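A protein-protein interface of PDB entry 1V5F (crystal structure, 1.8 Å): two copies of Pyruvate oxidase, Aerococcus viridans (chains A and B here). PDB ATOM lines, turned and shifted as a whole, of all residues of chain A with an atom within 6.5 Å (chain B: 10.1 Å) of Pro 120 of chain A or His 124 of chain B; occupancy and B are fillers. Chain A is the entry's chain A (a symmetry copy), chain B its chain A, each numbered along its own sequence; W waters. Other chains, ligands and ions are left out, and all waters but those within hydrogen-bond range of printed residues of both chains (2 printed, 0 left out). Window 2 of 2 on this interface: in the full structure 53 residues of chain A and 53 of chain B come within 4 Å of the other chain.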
ATOM      1  N   LEU A 116      -0.363  -4.301 -29.179  1.00  0.00           N
ATOM      2  CA  LEU A 116       0.483  -3.356 -28.461  1.00  0.00           C
ATOM      3  C   LEU A 116       1.950  -3.753 -28.499  1.00  0.00           C
ATOM      4  O   LEU A 116       2.291  -4.879 -28.854  1.00  0.00           O
ATOM      5  CB  LEU A 116       0.036  -3.260 -26.996  1.00  0.00           C
ATOM      6  CG  LEU A 116       0.459  -4.407 -26.064  1.00  0.00           C
ATOM      7  CD1 LEU A 116       0.057  -4.073 -24.634  1.00  0.00           C
ATOM      8  CD2 LEU A 116      -0.175  -5.717 -26.510  1.00  0.00           C
ATOM      9  N   ASN A 117       2.808  -2.807 -28.132  1.00  0.00           N
ATOM     10  CA  ASN A 117       4.249  -3.035 -28.081  1.00  0.00           C
ATOM     11  C   ASN A 117       4.538  -3.724 -26.747  1.00  0.00           C
ATOM     12  O   ASN A 117       4.429  -3.108 -25.686  1.00  0.00           O
ATOM     13  CB  ASN A 117       4.979  -1.690 -28.169  1.00  0.00           C
ATOM     14  CG  ASN A 117       6.477  -1.812 -27.964  1.00  0.00           C
ATOM     15  OD1 ASN A 117       7.045  -2.901 -28.043  1.00  0.00           O
ATOM     16  ND2 ASN A 117       7.131  -0.679 -27.716  1.00  0.00           N
ATOM     17  N   GLN A 118       4.899  -5.003 -26.803  1.00  0.00           N
ATOM     18  CA  GLN A 118       5.173  -5.759 -25.585  1.00  0.00           C
ATOM     19  C   GLN A 118       6.662  -5.866 -25.272  1.00  0.00           C
ATOM     20  O   GLN A 118       7.053  -6.562 -24.337  1.00  0.00           O
ATOM     21  CB  GLN A 118       4.578  -7.168 -25.696  1.00  0.00           C
ATOM     22  CG  GLN A 118       3.119  -7.195 -26.131  1.00  0.00           C
ATOM     23  CD  GLN A 118       2.567  -8.610 -26.239  1.00  0.00           C
ATOM     24  OE1 GLN A 118       2.095  -9.185 -25.258  1.00  0.00           O
ATOM     25  NE2 GLN A 118       2.636  -9.181 -27.439  1.00  0.00           N
ATOM     26  N   ASN A 119       7.492  -5.172 -26.042  1.00  0.00           N
ATOM     27  CA  ASN A 119       8.931  -5.226 -25.808  1.00  0.00           C
ATOM     28  C   ASN A 119       9.318  -4.616 -24.455  1.00  0.00           C
ATOM     29  O   ASN A 119      10.236  -5.102 -23.784  1.00  0.00           O
ATOM     30  CB  ASN A 119       9.679  -4.520 -26.939  1.00  0.00           C
ATOM     31  CG  ASN A 119      11.172  -4.765 -26.882  1.00  0.00           C
ATOM     32  OD1 ASN A 119      11.944  -3.887 -26.502  1.00  0.00           O
ATOM     33  ND2 ASN A 119      11.583  -5.973 -27.244  1.00  0.00           N
ATOM     34  N   PRO A 120       8.629  -3.540 -24.036  1.00  0.00           N
ATOM     35  CA  PRO A 120       8.957  -2.920 -22.747  1.00  0.00           C
ATOM     36  C   PRO A 120       8.593  -3.776 -21.534  1.00  0.00           C
ATOM     37  O   PRO A 120       9.233  -3.689 -20.488  1.00  0.00           O
ATOM     38  CB  PRO A 120       8.144  -1.626 -22.765  1.00  0.00           C
ATOM     39  CG  PRO A 120       8.044  -1.300 -24.223  1.00  0.00           C
ATOM     40  CD  PRO A 120       7.774  -2.647 -24.841  1.00  0.00           C
ATOM     41  N   MET A 121       7.568  -4.605 -21.691  1.00  0.00           N
ATOM     42  CA  MET A 121       7.057  -5.441 -20.608  1.00  0.00           C
ATOM     43  C   MET A 121       8.085  -6.151 -19.727  1.00  0.00           C
ATOM     44  O   MET A 121       8.027  -6.043 -18.498  1.00  0.00           O
ATOM     45  CB  MET A 121       6.066  -6.474 -21.168  1.00  0.00           C
ATOM     46  CG  MET A 121       5.149  -7.078 -20.112  1.00  0.00           C
ATOM     47  SD  MET A 121       3.906  -8.197 -20.802  1.00  0.00           S
ATOM     48  CE  MET A 121       2.806  -7.015 -21.645  1.00  0.00           C
ATOM     49  N   TYR A 122       9.025  -6.864 -20.340  1.00  0.00           N
ATOM     50  CA  TYR A 122      10.020  -7.605 -19.567  1.00  0.00           C
ATOM     51  C   TYR A 122      11.470  -7.249 -19.869  1.00  0.00           C
ATOM     52  O   TYR A 122      12.390  -7.979 -19.492  1.00  0.00           O
ATOM     53  CB  TYR A 122       9.810  -9.112 -19.771  1.00  0.00           C
ATOM     54  CG  TYR A 122       8.457  -9.596 -19.284  1.00  0.00           C
ATOM     55  CD1 TYR A 122       8.075  -9.416 -17.958  1.00  0.00           C
ATOM     56  CD2 TYR A 122       7.541 -10.186 -20.162  1.00  0.00           C
ATOM     57  CE1 TYR A 122       6.810  -9.801 -17.511  1.00  0.00           C
ATOM     58  CE2 TYR A 122       6.274 -10.576 -19.726  1.00  0.00           C
ATOM     59  CZ  TYR A 122       5.916 -10.376 -18.397  1.00  0.00           C
ATOM     60  OH  TYR A 122       4.666 -10.737 -17.951  1.00  0.00           O
ATOM     61  N   ASP A 123      11.689  -6.117 -20.517  1.00  0.00           N
ATOM     62  CA  ASP A 123      13.048  -5.733 -20.859  1.00  0.00           C
ATOM     63  C   ASP A 123      13.963  -5.573 -19.642  1.00  0.00           C
ATOM     64  O   ASP A 123      15.141  -5.920 -19.694  1.00  0.00           O
ATOM     65  CB  ASP A 123      13.045  -4.441 -21.669  1.00  0.00           C
ATOM     66  CG  ASP A 123      14.375  -4.184 -22.337  1.00  0.00           C
ATOM     67  OD1 ASP A 123      14.783  -5.027 -23.167  1.00  0.00           O
ATOM     68  OD2 ASP A 123      15.012  -3.156 -22.032  1.00  0.00           O
ATOM     69  N   HIS A 124      13.422  -5.055 -18.545  1.00  0.00           N
ATOM     70  CA  HIS A 124      14.220  -4.840 -17.344  1.00  0.00           C
ATOM     71  C   HIS A 124      14.784  -6.111 -16.705  1.00  0.00           C
ATOM     72  O   HIS A 124      15.902  -6.105 -16.199  1.00  0.00           O
ATOM     73  CB  HIS A 124      13.403  -4.073 -16.298  1.00  0.00           C
ATOM     74  CG  HIS A 124      14.160  -3.790 -15.038  1.00  0.00           C
ATOM     75  ND1 HIS A 124      15.250  -2.946 -14.999  1.00  0.00           N
ATOM     76  CD2 HIS A 124      14.017  -4.277 -13.782  1.00  0.00           C
ATOM     77  CE1 HIS A 124      15.747  -2.927 -13.775  1.00  0.00           C
ATOM     78  NE2 HIS A 124      15.017  -3.727 -13.017  1.00  0.00           N
ATOM     79  N   ASN A 129      15.474 -10.322 -25.018  1.00  0.00           N
ATOM     80  CA  ASN A 129      14.119  -9.786 -25.173  1.00  0.00           C
ATOM     81  C   ASN A 129      13.915  -9.212 -26.573  1.00  0.00           C
ATOM     82  O   ASN A 129      14.215  -8.045 -26.825  1.00  0.00           O
ATOM     83  CB  ASN A 129      13.888  -8.710 -24.108  1.00  0.00           C
ATOM     84  CG  ASN A 129      12.521  -8.076 -24.199  1.00  0.00           C
ATOM     85  OD1 ASN A 129      11.509  -8.770 -24.293  1.00  0.00           O
ATOM     86  ND2 ASN A 129      12.481  -6.745 -24.158  1.00  0.00           N
ATOM     87  N   ILE B  83      -0.496  -5.554 -12.785  1.00  0.00           N
ATOM     88  CA  ILE B  83      -0.337  -5.375 -14.229  1.00  0.00           C
ATOM     89  C   ILE B  83      -1.546  -5.482 -15.167  1.00  0.00           C
ATOM     90  O   ILE B  83      -1.786  -4.563 -15.951  1.00  0.00           O
ATOM     91  CB  ILE B  83       0.829  -6.259 -14.765  1.00  0.00           C
ATOM     92  CG1 ILE B  83       1.242  -5.774 -16.158  1.00  0.00           C
ATOM     93  CG2 ILE B  83       0.422  -7.724 -14.783  1.00  0.00           C
ATOM     94  CD1 ILE B  83       2.601  -6.281 -16.611  1.00  0.00           C
ATOM     95  N   LEU B  86      -3.767  -2.453 -14.625  1.00  0.00           N
ATOM     96  CA  LEU B  86      -3.180  -1.187 -15.052  1.00  0.00           C
ATOM     97  C   LEU B  86      -3.080  -1.057 -16.570  1.00  0.00           C
ATOM     98  O   LEU B  86      -3.296   0.029 -17.113  1.00  0.00           O
ATOM     99  CB  LEU B  86      -1.806  -0.990 -14.400  1.00  0.00           C
ATOM    100  CG  LEU B  86      -1.832  -1.010 -12.864  1.00  0.00           C
ATOM    101  CD1 LEU B  86      -0.458  -0.639 -12.323  1.00  0.00           C
ATOM    102  CD2 LEU B  86      -2.882  -0.034 -12.343  1.00  0.00           C
ATOM    103  N   TYR B  87      -2.749  -2.147 -17.259  1.00  0.00           N
ATOM    104  CA  TYR B  87      -2.666  -2.102 -18.717  1.00  0.00           C
ATOM    105  C   TYR B  87      -4.049  -1.829 -19.297  1.00  0.00           C
ATOM    106  O   TYR B  87      -4.188  -1.100 -20.280  1.00  0.00           O
ATOM    107  CB  TYR B  87      -2.114  -3.416 -19.271  1.00  0.00           C
ATOM    108  CG  TYR B  87      -0.642  -3.356 -19.622  1.00  0.00           C
ATOM    109  CD1 TYR B  87      -0.225  -3.247 -20.950  1.00  0.00           C
ATOM    110  CD2 TYR B  87       0.334  -3.392 -18.626  1.00  0.00           C
ATOM    111  CE1 TYR B  87       1.127  -3.175 -21.278  1.00  0.00           C
ATOM    112  CE2 TYR B  87       1.692  -3.318 -18.944  1.00  0.00           C
ATOM    113  CZ  TYR B  87       2.080  -3.210 -20.273  1.00  0.00           C
ATOM    114  OH  TYR B  87       3.419  -3.136 -20.598  1.00  0.00           O
ATOM    115  N   ALA B  90      -4.762   1.791 -18.860  1.00  0.00           N
ATOM    116  CA  ALA B  90      -3.920   2.571 -19.758  1.00  0.00           C
ATOM    117  C   ALA B  90      -4.491   2.601 -21.171  1.00  0.00           C
ATOM    118  O   ALA B  90      -4.568   3.661 -21.797  1.00  0.00           O
ATOM    119  CB  ALA B  90      -2.505   1.995 -19.776  1.00  0.00           C
ATOM    120  N   MET B  91      -4.896   1.438 -21.670  1.00  0.00           N
ATOM    121  CA  MET B  91      -5.445   1.358 -23.018  1.00  0.00           C
ATOM    122  C   MET B  91      -6.834   1.975 -23.135  1.00  0.00           C
ATOM    123  O   MET B  91      -7.206   2.464 -24.204  1.00  0.00           O
ATOM    124  CB  MET B  91      -5.449  -0.097 -23.499  1.00  0.00           C
ATOM    125  CG  MET B  91      -4.034  -0.658 -23.637  1.00  0.00           C
ATOM    126  SD  MET B  91      -3.886  -2.173 -24.606  1.00  0.00           S
ATOM    127  CE  MET B  91      -3.925  -1.507 -26.281  1.00  0.00           C
ATOM    128  N   GLN B 118      11.482  -0.907  -8.796  1.00  0.00           N
ATOM    129  CA  GLN B 118      10.179  -1.117  -9.417  1.00  0.00           C
ATOM    130  C   GLN B 118       9.779   0.012 -10.361  1.00  0.00           C
ATOM    131  O   GLN B 118       8.662   0.027 -10.876  1.00  0.00           O
ATOM    132  CB  GLN B 118       9.102  -1.278  -8.339  1.00  0.00           C
ATOM    133  CG  GLN B 118       9.449  -2.295  -7.259  1.00  0.00           C
ATOM    134  CD  GLN B 118       8.362  -2.420  -6.201  1.00  0.00           C
ATOM    135  OE1 GLN B 118       7.408  -3.184  -6.357  1.00  0.00           O
ATOM    136  NE2 GLN B 118       8.498  -1.656  -5.120  1.00  0.00           N
ATOM    137  N   ASN B 119      10.687   0.952 -10.598  1.00  0.00           N
ATOM    138  CA  ASN B 119      10.378   2.066 -11.487  1.00  0.00           C
ATOM    139  C   ASN B 119      10.150   1.605 -12.932  1.00  0.00           C
ATOM    140  O   ASN B 119       9.298   2.154 -13.641  1.00  0.00           O
ATOM    141  CB  ASN B 119      11.494   3.111 -11.435  1.00  0.00           C
ATOM    142  CG  ASN B 119      11.110   4.397 -12.135  1.00  0.00           C
ATOM    143  OD1 ASN B 119      11.579   4.686 -13.234  1.00  0.00           O
ATOM    144  ND2 ASN B 119      10.235   5.170 -11.504  1.00  0.00           N
ATOM    145  N   PRO B 120      10.910   0.596 -13.392  1.00  0.00           N
ATOM    146  CA  PRO B 120      10.730   0.114 -14.767  1.00  0.00           C
ATOM    147  C   PRO B 120       9.407  -0.614 -15.002  1.00  0.00           C
ATOM    148  O   PRO B 120       8.871  -0.603 -16.109  1.00  0.00           O
ATOM    149  CB  PRO B 120      11.915  -0.830 -14.964  1.00  0.00           C
ATOM    150  CG  PRO B 120      12.962  -0.266 -14.056  1.00  0.00           C
ATOM    151  CD  PRO B 120      12.171   0.085 -12.822  1.00  0.00           C
ATOM    152  N   MET B 121       8.887  -1.235 -13.950  1.00  0.00           N
ATOM    153  CA  MET B 121       7.663  -2.028 -14.028  1.00  0.00           C
ATOM    154  C   MET B 121       6.501  -1.445 -14.832  1.00  0.00           C
ATOM    155  O   MET B 121       5.956  -2.119 -15.712  1.00  0.00           O
ATOM    156  CB  MET B 121       7.178  -2.382 -12.614  1.00  0.00           C
ATOM    157  CG  MET B 121       6.205  -3.553 -12.574  1.00  0.00           C
ATOM    158  SD  MET B 121       5.739  -4.038 -10.895  1.00  0.00           S
ATOM    159  CE  MET B 121       7.288  -4.798 -10.312  1.00  0.00           C
ATOM    160  N   TYR B 122       6.125  -0.202 -14.546  1.00  0.00           N
ATOM    161  CA  TYR B 122       4.996   0.414 -15.241  1.00  0.00           C
ATOM    162  C   TYR B 122       5.313   1.717 -15.962  1.00  0.00           C
ATOM    163  O   TYR B 122       4.407   2.461 -16.348  1.00  0.00           O
ATOM    164  CB  TYR B 122       3.846   0.643 -14.249  1.00  0.00           C
ATOM    165  CG  TYR B 122       3.315  -0.642 -13.645  1.00  0.00           C
ATOM    166  CD1 TYR B 122       2.812  -1.654 -14.458  1.00  0.00           C
ATOM    167  CD2 TYR B 122       3.363  -0.867 -12.265  1.00  0.00           C
ATOM    168  CE1 TYR B 122       2.377  -2.866 -13.920  1.00  0.00           C
ATOM    169  CE2 TYR B 122       2.930  -2.074 -11.716  1.00  0.00           C
ATOM    170  CZ  TYR B 122       2.440  -3.070 -12.553  1.00  0.00           C
ATOM    171  OH  TYR B 122       2.024  -4.274 -12.034  1.00  0.00           O
ATOM    172  N   ASP B 123       6.589   1.989 -16.180  1.00  0.00           N
ATOM    173  CA  ASP B 123       6.959   3.229 -16.840  1.00  0.00           C
ATOM    174  C   ASP B 123       6.370   3.374 -18.246  1.00  0.00           C
ATOM    175  O   ASP B 123       5.987   4.469 -18.654  1.00  0.00           O
ATOM    176  CB  ASP B 123       8.477   3.360 -16.907  1.00  0.00           C
ATOM    177  CG  ASP B 123       8.913   4.762 -17.263  1.00  0.00           C
ATOM    178  OD1 ASP B 123       8.593   5.687 -16.484  1.00  0.00           O
ATOM    179  OD2 ASP B 123       9.562   4.941 -18.312  1.00  0.00           O
ATOM    180  N   HIS B 124       6.288   2.272 -18.982  1.00  0.00           N
ATOM    181  CA  HIS B 124       5.765   2.315 -20.342  1.00  0.00           C
ATOM    182  C   HIS B 124       4.299   2.738 -20.459  1.00  0.00           C
ATOM    183  O   HIS B 124       3.930   3.436 -21.398  1.00  0.00           O
ATOM    184  CB  HIS B 124       5.947   0.953 -21.021  1.00  0.00           C
ATOM    185  CG  HIS B 124       5.455   0.917 -22.434  1.00  0.00           C
ATOM    186  ND1 HIS B 124       6.043   1.649 -23.445  1.00  0.00           N
ATOM    187  CD2 HIS B 124       4.401   0.279 -22.996  1.00  0.00           C
ATOM    188  CE1 HIS B 124       5.370   1.465 -24.567  1.00  0.00           C
ATOM    189  NE2 HIS B 124       4.368   0.639 -24.322  1.00  0.00           N
ATOM    190  N   ILE B 125       3.467   2.336 -19.503  1.00  0.00           N
ATOM    191  CA  ILE B 125       2.040   2.658 -19.563  1.00  0.00           C
ATOM    192  C   ILE B 125       1.542   3.799 -18.675  1.00  0.00           C
ATOM    193  O   ILE B 125       0.422   4.278 -18.857  1.00  0.00           O
ATOM    194  CB  ILE B 125       1.192   1.424 -19.206  1.00  0.00           C
ATOM    195  CG1 ILE B 125       1.495   0.998 -17.766  1.00  0.00           C
ATOM    196  CG2 ILE B 125       1.496   0.281 -20.172  1.00  0.00           C
ATOM    197  CD1 ILE B 125       0.562  -0.061 -17.221  1.00  0.00           C
ATOM    198  N   ALA B 126       2.359   4.237 -17.724  1.00  0.00           N
ATOM    199  CA  ALA B 126       1.943   5.286 -16.795  1.00  0.00           C
ATOM    200  C   ALA B 126       2.029   6.729 -17.292  1.00  0.00           C
ATOM    201  O   ALA B 126       2.852   7.060 -18.147  1.00  0.00           O
ATOM    202  CB  ALA B 126       2.736   5.147 -15.496  1.00  0.00           C
ATOM    203  N   VAL B 127       1.161   7.583 -16.753  1.00  0.00           N
ATOM    204  CA  VAL B 127       1.173   9.002 -17.098  1.00  0.00           C
ATOM    205  C   VAL B 127       1.961   9.729 -16.011  1.00  0.00           C
ATOM    206  O   VAL B 127       2.258  10.917 -16.129  1.00  0.00           O
ATOM    207  CB  VAL B 127      -0.252   9.603 -17.168  1.00  0.00           C
ATOM    208  CG1 VAL B 127      -1.066   8.877 -18.226  1.00  0.00           C
ATOM    209  CG2 VAL B 127      -0.935   9.520 -15.803  1.00  0.00           C
ATOM    210  N   TYR B 128       2.299   8.987 -14.959  1.00  0.00           N
ATOM    211  CA  TYR B 128       3.055   9.495 -13.813  1.00  0.00           C
ATOM    212  C   TYR B 128       3.698   8.241 -13.195  1.00  0.00           C
ATOM    213  O   TYR B 128       3.009   7.257 -12.949  1.00  0.00           O
ATOM    214  CB  TYR B 128       2.087  10.146 -12.818  1.00  0.00           C
ATOM    215  CG  TYR B 128       2.716  11.049 -11.778  1.00  0.00           C
ATOM    216  CD1 TYR B 128       3.203  12.314 -12.122  1.00  0.00           C
ATOM    217  CD2 TYR B 128       2.763  10.669 -10.434  1.00  0.00           C
ATOM    218  CE1 TYR B 128       3.709  13.180 -11.154  1.00  0.00           C
ATOM    219  CE2 TYR B 128       3.269  11.524  -9.458  1.00  0.00           C
ATOM    220  CZ  TYR B 128       3.736  12.781  -9.825  1.00  0.00           C
ATOM    221  OH  TYR B 128       4.203  13.642  -8.860  1.00  0.00           O
ATOM    222  N   ASN B 129       5.008   8.263 -12.956  1.00  0.00           N
ATOM    223  CA  ASN B 129       5.675   7.081 -12.403  1.00  0.00           C
ATOM    224  C   ASN B 129       6.913   7.479 -11.601  1.00  0.00           C
ATOM    225  O   ASN B 129       8.004   7.617 -12.155  1.00  0.00           O
ATOM    226  CB  ASN B 129       6.053   6.144 -13.553  1.00  0.00           C
ATOM    227  CG  ASN B 129       6.772   4.901 -13.086  1.00  0.00           C
ATOM    228  OD1 ASN B 129       6.332   4.232 -12.151  1.00  0.00           O
ATOM    229  ND2 ASN B 129       7.881   4.575 -13.747  1.00  0.00           N
ATOM    230  N   VAL B 155      -2.989   5.910 -15.752  1.00  0.00           N
ATOM    231  CA  VAL B 155      -2.369   5.321 -14.568  1.00  0.00           C
ATOM    232  C   VAL B 155      -1.242   6.139 -13.936  1.00  0.00           C
ATOM    233  O   VAL B 155      -0.203   6.365 -14.561  1.00  0.00           O
ATOM    234  CB  VAL B 155      -1.813   3.914 -14.905  1.00  0.00           C
ATOM    235  CG1 VAL B 155      -1.218   3.266 -13.661  1.00  0.00           C
ATOM    236  CG2 VAL B 155      -2.919   3.043 -15.492  1.00  0.00           C
ATOM    237  N   VAL B 157       1.441   6.141 -11.010  1.00  0.00           N
ATOM    238  CA  VAL B 157       2.113   5.200 -10.113  1.00  0.00           C
ATOM    239  C   VAL B 157       3.137   5.817  -9.164  1.00  0.00           C
ATOM    240  O   VAL B 157       3.971   6.631  -9.569  1.00  0.00           O
ATOM    241  CB  VAL B 157       2.842   4.108 -10.927  1.00  0.00           C
ATOM    242  CG1 VAL B 157       3.333   2.998  -9.999  1.00  0.00           C
ATOM    243  CG2 VAL B 157       1.921   3.552 -12.004  1.00  0.00           C
ATOM    244  N   PHE B 411      -7.618  -3.947 -24.296  1.00  0.00           N
ATOM    245  CA  PHE B 411      -6.531  -4.783 -23.787  1.00  0.00           C
ATOM    246  C   PHE B 411      -7.150  -6.178 -23.718  1.00  0.00           C
ATOM    247  O   PHE B 411      -6.470  -7.193 -23.857  1.00  0.00           O
ATOM    248  CB  PHE B 411      -6.089  -4.317 -22.394  1.00  0.00           C
ATOM    249  CG  PHE B 411      -4.925  -5.097 -21.829  1.00  0.00           C
ATOM    250  CD1 PHE B 411      -3.710  -5.157 -22.513  1.00  0.00           C
ATOM    251  CD2 PHE B 411      -5.038  -5.755 -20.608  1.00  0.00           C
ATOM    252  CE1 PHE B 411      -2.628  -5.858 -21.989  1.00  0.00           C
ATOM    253  CE2 PHE B 411      -3.960  -6.460 -20.073  1.00  0.00           C
ATOM    254  CZ  PHE B 411      -2.749  -6.511 -20.767  1.00  0.00           C
HETATM  255  O   HOH W   1       2.428  -0.984 -25.514  1.00  0.00           O
HETATM  256  O   HOH W   2       4.937  -3.633 -22.842  1.00  0.00           O
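Pro 120 of chain A touches His 124 of chain B, and with the chains exchanged His 124 of chain A touches Pro 120 of chain B. Of the 4 pairs that touch across the chains among the printed residues, 2 have their exchanged pair printed and touching as well.
Tyr 87 of chain B touches Leu 116 of chain A. Asn 117 of chain A touches His 124 of chain B. CG of Pro 120 of chain A touches ND1 of His 124 of chain B (3.6 Å). Pro 120 of chain B touches His 124 of chain A (CG to ND1, 3.6 Å).
Hydrophobic or aromatic side chains of chain B that line the printed part of chain A: Tyr 87, Pro 120 and His 124. Of the 10 printed residues of chain A, 4 touch a printed residue of chain B.
Of chain B, only His 124 comes within 4 Å of Pro 120 of chain A. No residue of chain B comes within 4 Å of Asn 119 of chain A. Of the printed residues of chain B, His 124 of chain A touches Pro 120 (3.6 Å). Of the printed residues of chain B, Asn 117 of chain A touches His 124. Of the printed residues of chain A, Pro 120 of chain B touches His 124. Of the printed residues of chain B, Leu 116 of chain A touches Tyr 87 (3.6 Å). Tyr 122 of chain B touches none of the printed residues of chain A. Tyr 128 of chain B touches none of the printed residues of chain A. The nearest printed residue of chain A that does not touch His 124 of chain B is Met 121 of chain A (5.8 Å). The nearest printed residue of chain A that does not touch Pro 120 of chain B is Pro 120 of chain A (5.4 Å).
Water W2 lies within hydrogen-bond range of the side-chain hydroxyl of Tyr 87 of chain B (2.8 Å), the backbone carbonyl oxygen of Asn 117 of chain A (2.9 Å) and the backbone NH of Met 121 of chain A (3.0 Å). Water W1 bridges a ring nitrogen (NE2) of His 124 of chain B and the backbone carbonyl oxygen (O) of Asn 117 of chain A.
OD1 of Asn 117 of chain A lies within hydrogen-bond range of N of Asn 119 of chain A (3.1 Å).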
